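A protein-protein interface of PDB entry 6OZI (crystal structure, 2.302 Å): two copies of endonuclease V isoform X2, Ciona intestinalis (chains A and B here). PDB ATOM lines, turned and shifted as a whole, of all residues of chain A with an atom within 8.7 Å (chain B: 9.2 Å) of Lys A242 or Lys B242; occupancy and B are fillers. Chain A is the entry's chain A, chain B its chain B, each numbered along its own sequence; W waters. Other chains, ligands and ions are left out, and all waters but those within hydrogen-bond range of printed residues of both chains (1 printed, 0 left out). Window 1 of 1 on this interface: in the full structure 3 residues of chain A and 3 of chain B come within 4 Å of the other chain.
Among the printed residues, merely in contact across the chains: Lys A241 with Lys B242, Lys A242 with Lys B241, Lys A242 with Lys B242, Lys A242 with Glu B244 and Glu A244 with Lys B242.
NZ of Lys A241 is in salt-bridge range of OE1 of Glu A244 (2.7 Å).
Lys A241 touches Lys B242, and with the chains exchanged Lys A242 touches Lys B241. Lys A242 touches its own counterpart, Lys B242. Lys A242 touches Glu B244, and with the chains exchanged Glu A244 touches Lys B242. Positions printed for both chains: 48, 52, 54, 70, 72, 235, 236, 237, 238, 239, 240, 241, 242, 243 and 244.
Water W1 lies within hydrogen-bond range of O of Lys A241 and O of Lys B238.
Of the 17 printed residues of chain A, 3 touch a printed residue of chain B. Among the printed residues, 5 pairs touch across the chains. Among the printed residues, no Asp or Glu carboxylate lies within 4 Å of a Lys or Arg side-chain nitrogen of the other chain.
Lys A242 touches just these residues of chain B: Lys B241, Lys B242 and Glu B244. Lys B242 touches just these residues of chain A: Lys A241, Lys A242 and Glu A244. Printed residues of chain B within 4 Å of Lys A241: Lys B242. Printed residues of chain B within 4 Å of Glu A244: Lys B242. Of the printed residues of chain A, Glu B244 touches Lys A242 (3.2 Å). Of the printed residues of chain A, Lys B241 touches Lys A242 (3.6 Å). Ile A243 touches none of the printed residues of chain B. Thr B72 touches none of the printed residues of chain A. The nearest residue of chain B that does not touch Lys A242 is Ile B243 (5.8 Å). The nearest residue of chain A that does not touch Lys B242 is Ile A243 (5.9 Å). The nearest printed residue of chain A that does not touch Glu B244 is Lys A238 (6.2 Å).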
ATOM      1  N   SER A  44      26.459  18.907   9.314  1.00  0.00           N
ATOM      2  CA  SER A  44      25.709  19.336   8.150  1.00  0.00           C
ATOM      3  C   SER A  44      25.358  18.104   7.322  1.00  0.00           C
ATOM      4  O   SER A  44      26.115  17.132   7.289  1.00  0.00           O
ATOM      5  CB  SER A  44      26.532  20.325   7.323  1.00  0.00           C
ATOM      6  OG  SER A  44      25.834  20.762   6.174  1.00  0.00           O
ATOM      7  N   ILE A  48      19.984  16.161  -1.036  1.00  0.00           N
ATOM      8  CA  ILE A  48      20.100  15.521  -2.346  1.00  0.00           C
ATOM      9  C   ILE A  48      20.592  14.084  -2.199  1.00  0.00           C
ATOM     10  O   ILE A  48      19.934  13.134  -2.640  1.00  0.00           O
ATOM     11  CB  ILE A  48      21.033  16.342  -3.253  1.00  0.00           C
ATOM     12  CG1 ILE A  48      20.763  17.839  -3.065  1.00  0.00           C
ATOM     13  CG2 ILE A  48      20.859  15.938  -4.707  1.00  0.00           C
ATOM     14  CD1 ILE A  48      21.818  18.748  -3.682  1.00  0.00           C
ATOM     15  N   ASN A  49      21.771  13.910  -1.595  1.00  0.00           N
ATOM     16  CA  ASN A  49      22.355  12.602  -1.298  1.00  0.00           C
ATOM     17  C   ASN A  49      22.223  12.378   0.203  1.00  0.00           C
ATOM     18  O   ASN A  49      23.021  12.901   0.985  1.00  0.00           O
ATOM     19  CB  ASN A  49      23.818  12.533  -1.725  1.00  0.00           C
ATOM     20  CG  ASN A  49      24.129  13.441  -2.900  1.00  0.00           C
ATOM     21  OD1 ASN A  49      23.958  13.057  -4.056  1.00  0.00           O
ATOM     22  ND2 ASN A  49      24.594  14.651  -2.607  1.00  0.00           N
ATOM     23  N   LEU A  52      25.226  11.500   2.477  1.00  0.00           N
ATOM     24  CA  LEU A  52      26.361  12.409   2.552  1.00  0.00           C
ATOM     25  C   LEU A  52      26.186  13.413   3.689  1.00  0.00           C
ATOM     26  O   LEU A  52      25.184  14.134   3.743  1.00  0.00           O
ATOM     27  CB  LEU A  52      26.525  13.115   1.209  1.00  0.00           C
ATOM     28  CG  LEU A  52      27.403  14.353   1.176  1.00  0.00           C
ATOM     29  CD1 LEU A  52      28.834  13.940   1.476  1.00  0.00           C
ATOM     30  CD2 LEU A  52      27.311  15.022  -0.182  1.00  0.00           C
ATOM     31  N   VAL A  54      28.692  15.946   6.753  1.00  0.00           N
ATOM     32  CA  VAL A  54      29.990  16.467   7.171  1.00  0.00           C
ATOM     33  C   VAL A  54      29.892  16.868   8.638  1.00  0.00           C
ATOM     34  O   VAL A  54      29.022  17.661   9.007  1.00  0.00           O
ATOM     35  CB  VAL A  54      30.432  17.675   6.325  1.00  0.00           C
ATOM     36  CG1 VAL A  54      31.681  18.302   6.910  1.00  0.00           C
ATOM     37  CG2 VAL A  54      30.652  17.273   4.871  1.00  0.00           C
ATOM     38  N   MET A  70      40.116  23.706  13.968  1.00  0.00           N
ATOM     39  CA  MET A  70      38.947  23.358  13.175  1.00  0.00           C
ATOM     40  C   MET A  70      39.246  22.091  12.389  1.00  0.00           C
ATOM     41  O   MET A  70      40.361  21.910  11.894  1.00  0.00           O
ATOM     42  CB  MET A  70      38.547  24.492  12.221  1.00  0.00           C
ATOM     43  CG  MET A  70      37.241  24.246  11.461  1.00  0.00           C
ATOM     44  SD  MET A  70      37.460  23.331   9.914  1.00  0.00           S
ATOM     45  CE  MET A  70      37.931  24.664   8.809  1.00  0.00           C
ATOM     46  N   THR A  72      36.842  19.244   9.697  1.00  0.00           N
ATOM     47  CA  THR A  72      35.603  18.702   9.152  1.00  0.00           C
ATOM     48  C   THR A  72      35.870  17.300   8.625  1.00  0.00           C
ATOM     49  O   THR A  72      36.976  16.993   8.189  1.00  0.00           O
ATOM     50  CB  THR A  72      35.030  19.567   8.015  1.00  0.00           C
ATOM     51  OG1 THR A  72      35.961  19.605   6.925  1.00  0.00           O
ATOM     52  CG2 THR A  72      34.764  20.986   8.493  1.00  0.00           C
ATOM     53  N   TRP A 235      31.472  25.926   9.306  1.00  0.00           N
ATOM     54  CA  TRP A 235      32.459  25.154   8.553  1.00  0.00           C
ATOM     55  C   TRP A 235      31.892  23.809   8.107  1.00  0.00           C
ATOM     56  O   TRP A 235      32.194  23.345   6.994  1.00  0.00           O
ATOM     57  CB  TRP A 235      33.742  24.964   9.365  1.00  0.00           C
ATOM     58  CG  TRP A 235      34.389  26.259   9.855  1.00  0.00           C
ATOM     59  CD1 TRP A 235      34.696  26.575  11.147  1.00  0.00           C
ATOM     60  CD2 TRP A 235      34.776  27.399   9.065  1.00  0.00           C
ATOM     61  NE1 TRP A 235      35.266  27.822  11.207  1.00  0.00           N
ATOM     62  CE2 TRP A 235      35.321  28.351   9.947  1.00  0.00           C
ATOM     63  CE3 TRP A 235      34.722  27.702   7.698  1.00  0.00           C
ATOM     64  CZ2 TRP A 235      35.810  29.581   9.511  1.00  0.00           C
ATOM     65  CZ3 TRP A 235      35.209  28.931   7.266  1.00  0.00           C
ATOM     66  CH2 TRP A 235      35.743  29.853   8.171  1.00  0.00           C
ATOM     67  N   SER A 236      31.072  23.163   8.949  1.00  0.00           N
ATOM     68  CA  SER A 236      30.450  21.917   8.503  1.00  0.00           C
ATOM     69  C   SER A 236      29.603  22.151   7.254  1.00  0.00           C
ATOM     70  O   SER A 236      29.707  21.399   6.270  1.00  0.00           O
ATOM     71  CB  SER A 236      29.614  21.296   9.623  1.00  0.00           C
ATOM     72  OG  SER A 236      28.488  22.095   9.924  1.00  0.00           O
ATOM     73  N   ARG A 237      28.792  23.224   7.258  1.00  0.00           N
ATOM     74  CA  ARG A 237      27.912  23.499   6.119  1.00  0.00           C
ATOM     75  C   ARG A 237      28.711  23.823   4.863  1.00  0.00           C
ATOM     76  O   ARG A 237      28.412  23.318   3.771  1.00  0.00           O
ATOM     77  CB  ARG A 237      26.989  24.677   6.429  1.00  0.00           C
ATOM     78  CG  ARG A 237      26.036  24.991   5.281  1.00  0.00           C
ATOM     79  CD  ARG A 237      25.311  26.326   5.447  1.00  0.00           C
ATOM     80  NE  ARG A 237      24.697  26.529   6.751  1.00  0.00           N
ATOM     81  CZ  ARG A 237      25.117  27.459   7.610  1.00  0.00           C
ATOM     82  NH1 ARG A 237      26.131  28.258   7.280  1.00  0.00           N
ATOM     83  NH2 ARG A 237      24.521  27.605   8.789  1.00  0.00           N
ATOM     84  N   LYS A 238      29.730  24.671   5.003  1.00  0.00           N
ATOM     85  CA  LYS A 238      30.519  25.091   3.851  1.00  0.00           C
ATOM     86  C   LYS A 238      31.208  23.898   3.207  1.00  0.00           C
ATOM     87  O   LYS A 238      31.167  23.727   1.979  1.00  0.00           O
ATOM     88  CB  LYS A 238      31.532  26.154   4.285  1.00  0.00           C
ATOM     89  CG  LYS A 238      32.531  26.565   3.218  1.00  0.00           C
ATOM     90  CD  LYS A 238      33.484  27.626   3.759  1.00  0.00           C
ATOM     91  CE  LYS A 238      34.575  27.970   2.751  1.00  0.00           C
ATOM     92  NZ  LYS A 238      35.443  29.086   3.234  1.00  0.00           N
ATOM     93  N   GLU A 239      31.828  23.044   4.023  1.00  0.00           N
ATOM     94  CA  GLU A 239      32.464  21.868   3.457  1.00  0.00           C
ATOM     95  C   GLU A 239      31.437  20.960   2.794  1.00  0.00           C
ATOM     96  O   GLU A 239      31.697  20.413   1.718  1.00  0.00           O
ATOM     97  CB  GLU A 239      33.250  21.111   4.526  1.00  0.00           C
ATOM     98  CG  GLU A 239      33.934  19.841   4.007  1.00  0.00           C
ATOM     99  CD  GLU A 239      35.051  20.117   3.011  1.00  0.00           C
ATOM    100  OE1 GLU A 239      35.514  21.274   2.916  1.00  0.00           O
ATOM    101  OE2 GLU A 239      35.475  19.167   2.315  1.00  0.00           O
ATOM    102  N   LEU A 240      30.246  20.822   3.388  1.00  0.00           N
ATOM    103  CA  LEU A 240      29.230  19.990   2.745  1.00  0.00           C
ATOM    104  C   LEU A 240      28.860  20.537   1.369  1.00  0.00           C
ATOM    105  O   LEU A 240      28.785  19.786   0.388  1.00  0.00           O
ATOM    106  CB  LEU A 240      27.981  19.878   3.622  1.00  0.00           C
ATOM    107  CG  LEU A 240      26.880  19.093   2.896  1.00  0.00           C
ATOM    108  CD1 LEU A 240      27.088  17.594   3.020  1.00  0.00           C
ATOM    109  CD2 LEU A 240      25.520  19.476   3.389  1.00  0.00           C
ATOM    110  N   LYS A 241      28.650  21.855   1.273  1.00  0.00           N
ATOM    111  CA  LYS A 241      28.320  22.453  -0.015  1.00  0.00           C
ATOM    112  C   LYS A 241      29.451  22.308  -1.022  1.00  0.00           C
ATOM    113  O   LYS A 241      29.191  22.262  -2.229  1.00  0.00           O
ATOM    114  CB  LYS A 241      27.955  23.929   0.152  1.00  0.00           C
ATOM    115  CG  LYS A 241      26.464  24.197   0.050  1.00  0.00           C
ATOM    116  CD  LYS A 241      25.694  23.579   1.199  1.00  0.00           C
ATOM    117  CE  LYS A 241      24.196  23.746   0.986  1.00  0.00           C
ATOM    118  NZ  LYS A 241      23.724  22.989  -0.218  1.00  0.00           N
ATOM    119  N   LYS A 242      30.703  22.239  -0.563  1.00  0.00           N
ATOM    120  CA  LYS A 242      31.795  22.066  -1.520  1.00  0.00           C
ATOM    121  C   LYS A 242      31.756  20.694  -2.184  1.00  0.00           C
ATOM    122  O   LYS A 242      31.966  20.585  -3.397  1.00  0.00           O
ATOM    123  CB  LYS A 242      33.145  22.291  -0.840  1.00  0.00           C
ATOM    124  CG  LYS A 242      33.649  23.712  -0.964  1.00  0.00           C
ATOM    125  CD  LYS A 242      34.891  23.934  -0.122  1.00  0.00           C
ATOM    126  CE  LYS A 242      35.050  25.409   0.240  1.00  0.00           C
ATOM    127  NZ  LYS A 242      36.238  25.643   1.114  1.00  0.00           N
ATOM    128  N   ILE A 243      31.460  19.641  -1.419  1.00  0.00           N
ATOM    129  CA  ILE A 243      31.520  18.272  -1.928  1.00  0.00           C
ATOM    130  C   ILE A 243      30.169  17.744  -2.372  1.00  0.00           C
ATOM    131  O   ILE A 243      30.088  16.604  -2.844  1.00  0.00           O
ATOM    132  CB  ILE A 243      32.116  17.319  -0.872  1.00  0.00           C
ATOM    133  CG1 ILE A 243      31.143  17.158   0.300  1.00  0.00           C
ATOM    134  CG2 ILE A 243      33.452  17.840  -0.384  1.00  0.00           C
ATOM    135  CD1 ILE A 243      31.715  16.386   1.460  1.00  0.00           C
ATOM    136  N   GLU A 244      29.107  18.522  -2.227  1.00  0.00           N
ATOM    137  CA  GLU A 244      27.775  18.036  -2.556  1.00  0.00           C
ATOM    138  C   GLU A 244      27.650  17.806  -4.055  1.00  0.00           C
ATOM    139  O   GLU A 244      28.185  18.570  -4.861  1.00  0.00           O
ATOM    140  CB  GLU A 244      26.719  19.026  -2.069  1.00  0.00           C
ATOM    141  CG  GLU A 244      25.297  18.502  -2.081  1.00  0.00           C
ATOM    142  CD  GLU A 244      24.363  19.388  -1.274  1.00  0.00           C
ATOM    143  OE1 GLU A 244      24.674  20.591  -1.121  1.00  0.00           O
ATOM    144  OE2 GLU A 244      23.331  18.881  -0.783  1.00  0.00           O
ATOM    145  OXT GLU A 244      27.021  16.841  -4.493  1.00  0.00           O
ATOM    146  N   SER B  46      33.411  35.476  -6.539  1.00  0.00           N
ATOM    147  CA  SER B  46      34.034  35.093  -5.285  1.00  0.00           C
ATOM    148  C   SER B  46      34.806  36.288  -4.750  1.00  0.00           C
ATOM    149  O   SER B  46      35.501  36.975  -5.503  1.00  0.00           O
ATOM    150  CB  SER B  46      34.963  33.890  -5.467  1.00  0.00           C
ATOM    151  OG  SER B  46      35.426  33.410  -4.214  1.00  0.00           O
ATOM    152  N   ILE B  48      37.056  35.770  -2.328  1.00  0.00           N
ATOM    153  CA  ILE B  48      38.397  35.231  -2.115  1.00  0.00           C
ATOM    154  C   ILE B  48      39.237  35.402  -3.376  1.00  0.00           C
ATOM    155  O   ILE B  48      40.357  35.926  -3.335  1.00  0.00           O
ATOM    156  CB  ILE B  48      38.327  33.752  -1.692  1.00  0.00           C
ATOM    157  CG1 ILE B  48      37.179  33.527  -0.705  1.00  0.00           C
ATOM    158  CG2 ILE B  48      39.654  33.312  -1.084  1.00  0.00           C
ATOM    159  CD1 ILE B  48      36.849  32.062  -0.466  1.00  0.00           C
ATOM    160  N   LEU B  52      37.775  34.738 -10.398  1.00  0.00           N
ATOM    161  CA  LEU B  52      36.920  33.554 -10.414  1.00  0.00           C
ATOM    162  C   LEU B  52      35.444  33.935 -10.272  1.00  0.00           C
ATOM    163  O   LEU B  52      35.045  34.540  -9.269  1.00  0.00           O
ATOM    164  CB  LEU B  52      37.336  32.611  -9.290  1.00  0.00           C
ATOM    165  CG  LEU B  52      36.308  31.557  -8.884  1.00  0.00           C
ATOM    166  CD1 LEU B  52      36.003  30.639 -10.054  1.00  0.00           C
ATOM    167  CD2 LEU B  52      36.810  30.765  -7.686  1.00  0.00           C
ATOM    168  N   VAL B  54      31.116  32.714 -11.811  1.00  0.00           N
ATOM    169  CA  VAL B  54      30.233  31.741 -12.454  1.00  0.00           C
ATOM    170  C   VAL B  54      29.028  32.481 -13.019  1.00  0.00           C
ATOM    171  O   VAL B  54      28.294  33.133 -12.273  1.00  0.00           O
ATOM    172  CB  VAL B  54      29.763  30.642 -11.482  1.00  0.00           C
ATOM    173  CG1 VAL B  54      28.655  29.807 -12.109  1.00  0.00           C
ATOM    174  CG2 VAL B  54      30.926  29.748 -11.092  1.00  0.00           C
ATOM    175  N   MET B  70      18.481  25.744 -17.926  1.00  0.00           N
ATOM    176  CA  MET B  70      19.470  26.254 -16.987  1.00  0.00           C
ATOM    177  C   MET B  70      20.862  25.901 -17.491  1.00  0.00           C
ATOM    178  O   MET B  70      21.078  24.807 -18.019  1.00  0.00           O
ATOM    179  CB  MET B  70      19.252  25.684 -15.582  1.00  0.00           C
ATOM    180  CG  MET B  70      20.159  26.294 -14.532  1.00  0.00           C
ATOM    181  SD  MET B  70      21.762  25.482 -14.399  1.00  0.00           S
ATOM    182  CE  MET B  70      21.350  24.114 -13.315  1.00  0.00           C
ATOM    183  N   THR B  72      25.211  26.906 -16.310  1.00  0.00           N
ATOM    184  CA  THR B  72      26.230  27.669 -15.602  1.00  0.00           C
ATOM    185  C   THR B  72      27.574  27.513 -16.297  1.00  0.00           C
ATOM    186  O   THR B  72      27.860  26.487 -16.914  1.00  0.00           O
ATOM    187  CB  THR B  72      26.356  27.247 -14.126  1.00  0.00           C
ATOM    188  OG1 THR B  72      26.722  25.862 -14.036  1.00  0.00           O
ATOM    189  CG2 THR B  72      25.050  27.488 -13.384  1.00  0.00           C
ATOM    190  N   LYS B 234      20.317  31.734  -7.958  1.00  0.00           N
ATOM    191  CA  LYS B 234      20.394  30.502  -7.177  1.00  0.00           C
ATOM    192  C   LYS B 234      21.429  29.544  -7.754  1.00  0.00           C
ATOM    193  O   LYS B 234      22.318  29.056  -7.039  1.00  0.00           O
ATOM    194  CB  LYS B 234      19.015  29.846  -7.161  1.00  0.00           C
ATOM    195  CG  LYS B 234      18.915  28.463  -6.519  1.00  0.00           C
ATOM    196  CD  LYS B 234      17.472  27.975  -6.670  1.00  0.00           C
ATOM    197  CE  LYS B 234      17.039  27.052  -5.555  1.00  0.00           C
ATOM    198  NZ  LYS B 234      17.385  25.623  -5.794  1.00  0.00           N
ATOM    199  N   TRP B 235      21.311  29.235  -9.048  1.00  0.00           N
ATOM    200  CA  TRP B 235      22.214  28.253  -9.635  1.00  0.00           C
ATOM    201  C   TRP B 235      23.632  28.800  -9.742  1.00  0.00           C
ATOM    202  O   TRP B 235      24.599  28.080  -9.458  1.00  0.00           O
ATOM    203  CB  TRP B 235      21.690  27.806 -10.998  1.00  0.00           C
ATOM    204  CG  TRP B 235      20.301  27.268 -10.903  1.00  0.00           C
ATOM    205  CD1 TRP B 235      19.199  27.724 -11.565  1.00  0.00           C
ATOM    206  CD2 TRP B 235      19.851  26.183 -10.075  1.00  0.00           C
ATOM    207  NE1 TRP B 235      18.095  26.988 -11.210  1.00  0.00           N
ATOM    208  CE2 TRP B 235      18.468  26.033 -10.300  1.00  0.00           C
ATOM    209  CE3 TRP B 235      20.486  25.319  -9.172  1.00  0.00           C
ATOM    210  CZ2 TRP B 235      17.706  25.057  -9.657  1.00  0.00           C
ATOM    211  CZ3 TRP B 235      19.729  24.348  -8.537  1.00  0.00           C
ATOM    212  CH2 TRP B 235      18.353  24.227  -8.780  1.00  0.00           C
ATOM    213  N   SER B 236      23.780  30.075 -10.116  1.00  0.00           N
ATOM    214  CA  SER B 236      25.126  30.635 -10.162  1.00  0.00           C
ATOM    215  C   SER B 236      25.791  30.562  -8.792  1.00  0.00           C
ATOM    216  O   SER B 236      26.953  30.157  -8.677  1.00  0.00           O
ATOM    217  CB  SER B 236      25.100  32.070 -10.688  1.00  0.00           C
ATOM    218  OG  SER B 236      24.456  32.953  -9.796  1.00  0.00           O
ATOM    219  N   ARG B 237      25.061  30.921  -7.735  1.00  0.00           N
ATOM    220  CA  ARG B 237      25.656  30.875  -6.405  1.00  0.00           C
ATOM    221  C   ARG B 237      26.007  29.449  -5.989  1.00  0.00           C
ATOM    222  O   ARG B 237      27.091  29.205  -5.441  1.00  0.00           O
ATOM    223  CB  ARG B 237      24.737  31.548  -5.388  1.00  0.00           C
ATOM    224  CG  ARG B 237      25.144  31.281  -3.937  1.00  0.00           C
ATOM    225  CD  ARG B 237      24.265  32.042  -2.969  1.00  0.00           C
ATOM    226  NE  ARG B 237      24.368  33.478  -3.242  1.00  0.00           N
ATOM    227  CZ  ARG B 237      23.393  34.255  -3.709  1.00  0.00           C
ATOM    228  NH1 ARG B 237      22.187  33.760  -3.958  1.00  0.00           N
ATOM    229  NH2 ARG B 237      23.625  35.548  -3.912  1.00  0.00           N
ATOM    230  N   LYS B 238      25.115  28.486  -6.241  1.00  0.00           N
ATOM    231  CA  LYS B 238      25.420  27.114  -5.839  1.00  0.00           C
ATOM    232  C   LYS B 238      26.663  26.591  -6.558  1.00  0.00           C
ATOM    233  O   LYS B 238      27.578  26.034  -5.931  1.00  0.00           O
ATOM    234  CB  LYS B 238      24.218  26.205  -6.099  1.00  0.00           C
ATOM    235  CG  LYS B 238      24.495  24.730  -5.833  1.00  0.00           C
ATOM    236  CD  LYS B 238      23.251  23.869  -6.025  1.00  0.00           C
ATOM    237  CE  LYS B 238      22.349  23.884  -4.783  1.00  0.00           C
ATOM    238  NZ  LYS B 238      21.566  25.160  -4.621  1.00  0.00           N
ATOM    239  N   GLU B 239      26.727  26.790  -7.876  1.00  0.00           N
ATOM    240  CA  GLU B 239      27.885  26.320  -8.629  1.00  0.00           C
ATOM    241  C   GLU B 239      29.166  27.021  -8.185  1.00  0.00           C
ATOM    242  O   GLU B 239      30.229  26.396  -8.119  1.00  0.00           O
ATOM    243  CB  GLU B 239      27.632  26.503 -10.123  1.00  0.00           C
ATOM    244  CG  GLU B 239      28.764  26.037 -11.008  1.00  0.00           C
ATOM    245  CD  GLU B 239      28.981  24.530 -10.934  1.00  0.00           C
ATOM    246  OE1 GLU B 239      28.103  23.801 -10.419  1.00  0.00           O
ATOM    247  OE2 GLU B 239      30.048  24.080 -11.395  1.00  0.00           O
ATOM    248  N   LEU B 240      29.086  28.318  -7.873  1.00  0.00           N
ATOM    249  CA  LEU B 240      30.256  29.022  -7.352  1.00  0.00           C
ATOM    250  C   LEU B 240      30.729  28.418  -6.037  1.00  0.00           C
ATOM    251  O   LEU B 240      31.936  28.279  -5.809  1.00  0.00           O
ATOM    252  CB  LEU B 240      29.947  30.507  -7.162  1.00  0.00           C
ATOM    253  CG  LEU B 240      31.085  31.292  -6.497  1.00  0.00           C
ATOM    254  CD1 LEU B 240      32.155  31.676  -7.516  1.00  0.00           C
ATOM    255  CD2 LEU B 240      30.554  32.511  -5.773  1.00  0.00           C
ATOM    256  N   LYS B 241      29.794  28.091  -5.141  1.00  0.00           N
ATOM    257  CA  LYS B 241      30.173  27.467  -3.877  1.00  0.00           C
ATOM    258  C   LYS B 241      30.817  26.106  -4.101  1.00  0.00           C
ATOM    259  O   LYS B 241      31.648  25.674  -3.294  1.00  0.00           O
ATOM    260  CB  LYS B 241      28.949  27.326  -2.971  1.00  0.00           C
ATOM    261  CG  LYS B 241      28.856  28.365  -1.876  1.00  0.00           C
ATOM    262  CD  LYS B 241      28.624  29.748  -2.450  1.00  0.00           C
ATOM    263  CE  LYS B 241      28.630  30.803  -1.351  1.00  0.00           C
ATOM    264  NZ  LYS B 241      29.959  30.895  -0.684  1.00  0.00           N
ATOM    265  N   LYS B 242      30.458  25.421  -5.195  1.00  0.00           N
ATOM    266  CA  LYS B 242      31.086  24.133  -5.486  1.00  0.00           C
ATOM    267  C   LYS B 242      32.567  24.291  -5.817  1.00  0.00           C
ATOM    268  O   LYS B 242      33.386  23.454  -5.421  1.00  0.00           O
ATOM    269  CB  LYS B 242      30.349  23.426  -6.625  1.00  0.00           C
ATOM    270  CG  LYS B 242      29.278  22.459  -6.139  1.00  0.00           C
ATOM    271  CD  LYS B 242      28.421  21.926  -7.275  1.00  0.00           C
ATOM    272  CE  LYS B 242      27.060  21.469  -6.754  1.00  0.00           C
ATOM    273  NZ  LYS B 242      26.157  20.997  -7.847  1.00  0.00           N
ATOM    274  N   ILE B 243      32.934  25.336  -6.552  1.00  0.00           N
ATOM    275  CA  ILE B 243      34.324  25.550  -6.945  1.00  0.00           C
ATOM    276  C   ILE B 243      35.024  26.538  -6.007  1.00  0.00           C
ATOM    277  O   ILE B 243      36.039  27.130  -6.377  1.00  0.00           O
ATOM    278  CB  ILE B 243      34.438  25.986  -8.414  1.00  0.00           C
ATOM    279  CG1 ILE B 243      33.866  27.393  -8.615  1.00  0.00           C
ATOM    280  CG2 ILE B 243      33.737  24.984  -9.327  1.00  0.00           C
ATOM    281  CD1 ILE B 243      33.800  27.812 -10.071  1.00  0.00           C
ATOM    282  N   GLU B 244      34.492  26.714  -4.794  1.00  0.00           N
ATOM    283  CA  GLU B 244      35.039  27.564  -3.721  1.00  0.00           C
ATOM    284  C   GLU B 244      34.805  29.059  -3.974  1.00  0.00           C
ATOM    285  O   GLU B 244      35.265  29.622  -4.968  1.00  0.00           O
ATOM    286  CB  GLU B 244      36.536  27.292  -3.503  1.00  0.00           C
ATOM    287  CG  GLU B 244      36.848  25.961  -2.823  1.00  0.00           C
ATOM    288  CD  GLU B 244      36.581  24.748  -3.711  1.00  0.00           C
ATOM    289  OE1 GLU B 244      37.115  24.697  -4.840  1.00  0.00           O
ATOM    290  OE2 GLU B 244      35.835  23.841  -3.281  1.00  0.00           O
ATOM    291  OXT GLU B 244      34.151  29.751  -3.184  1.00  0.00           O
HETATM  292  O   HOH W   1      26.882  23.867  -3.498  1.00  0.00           O
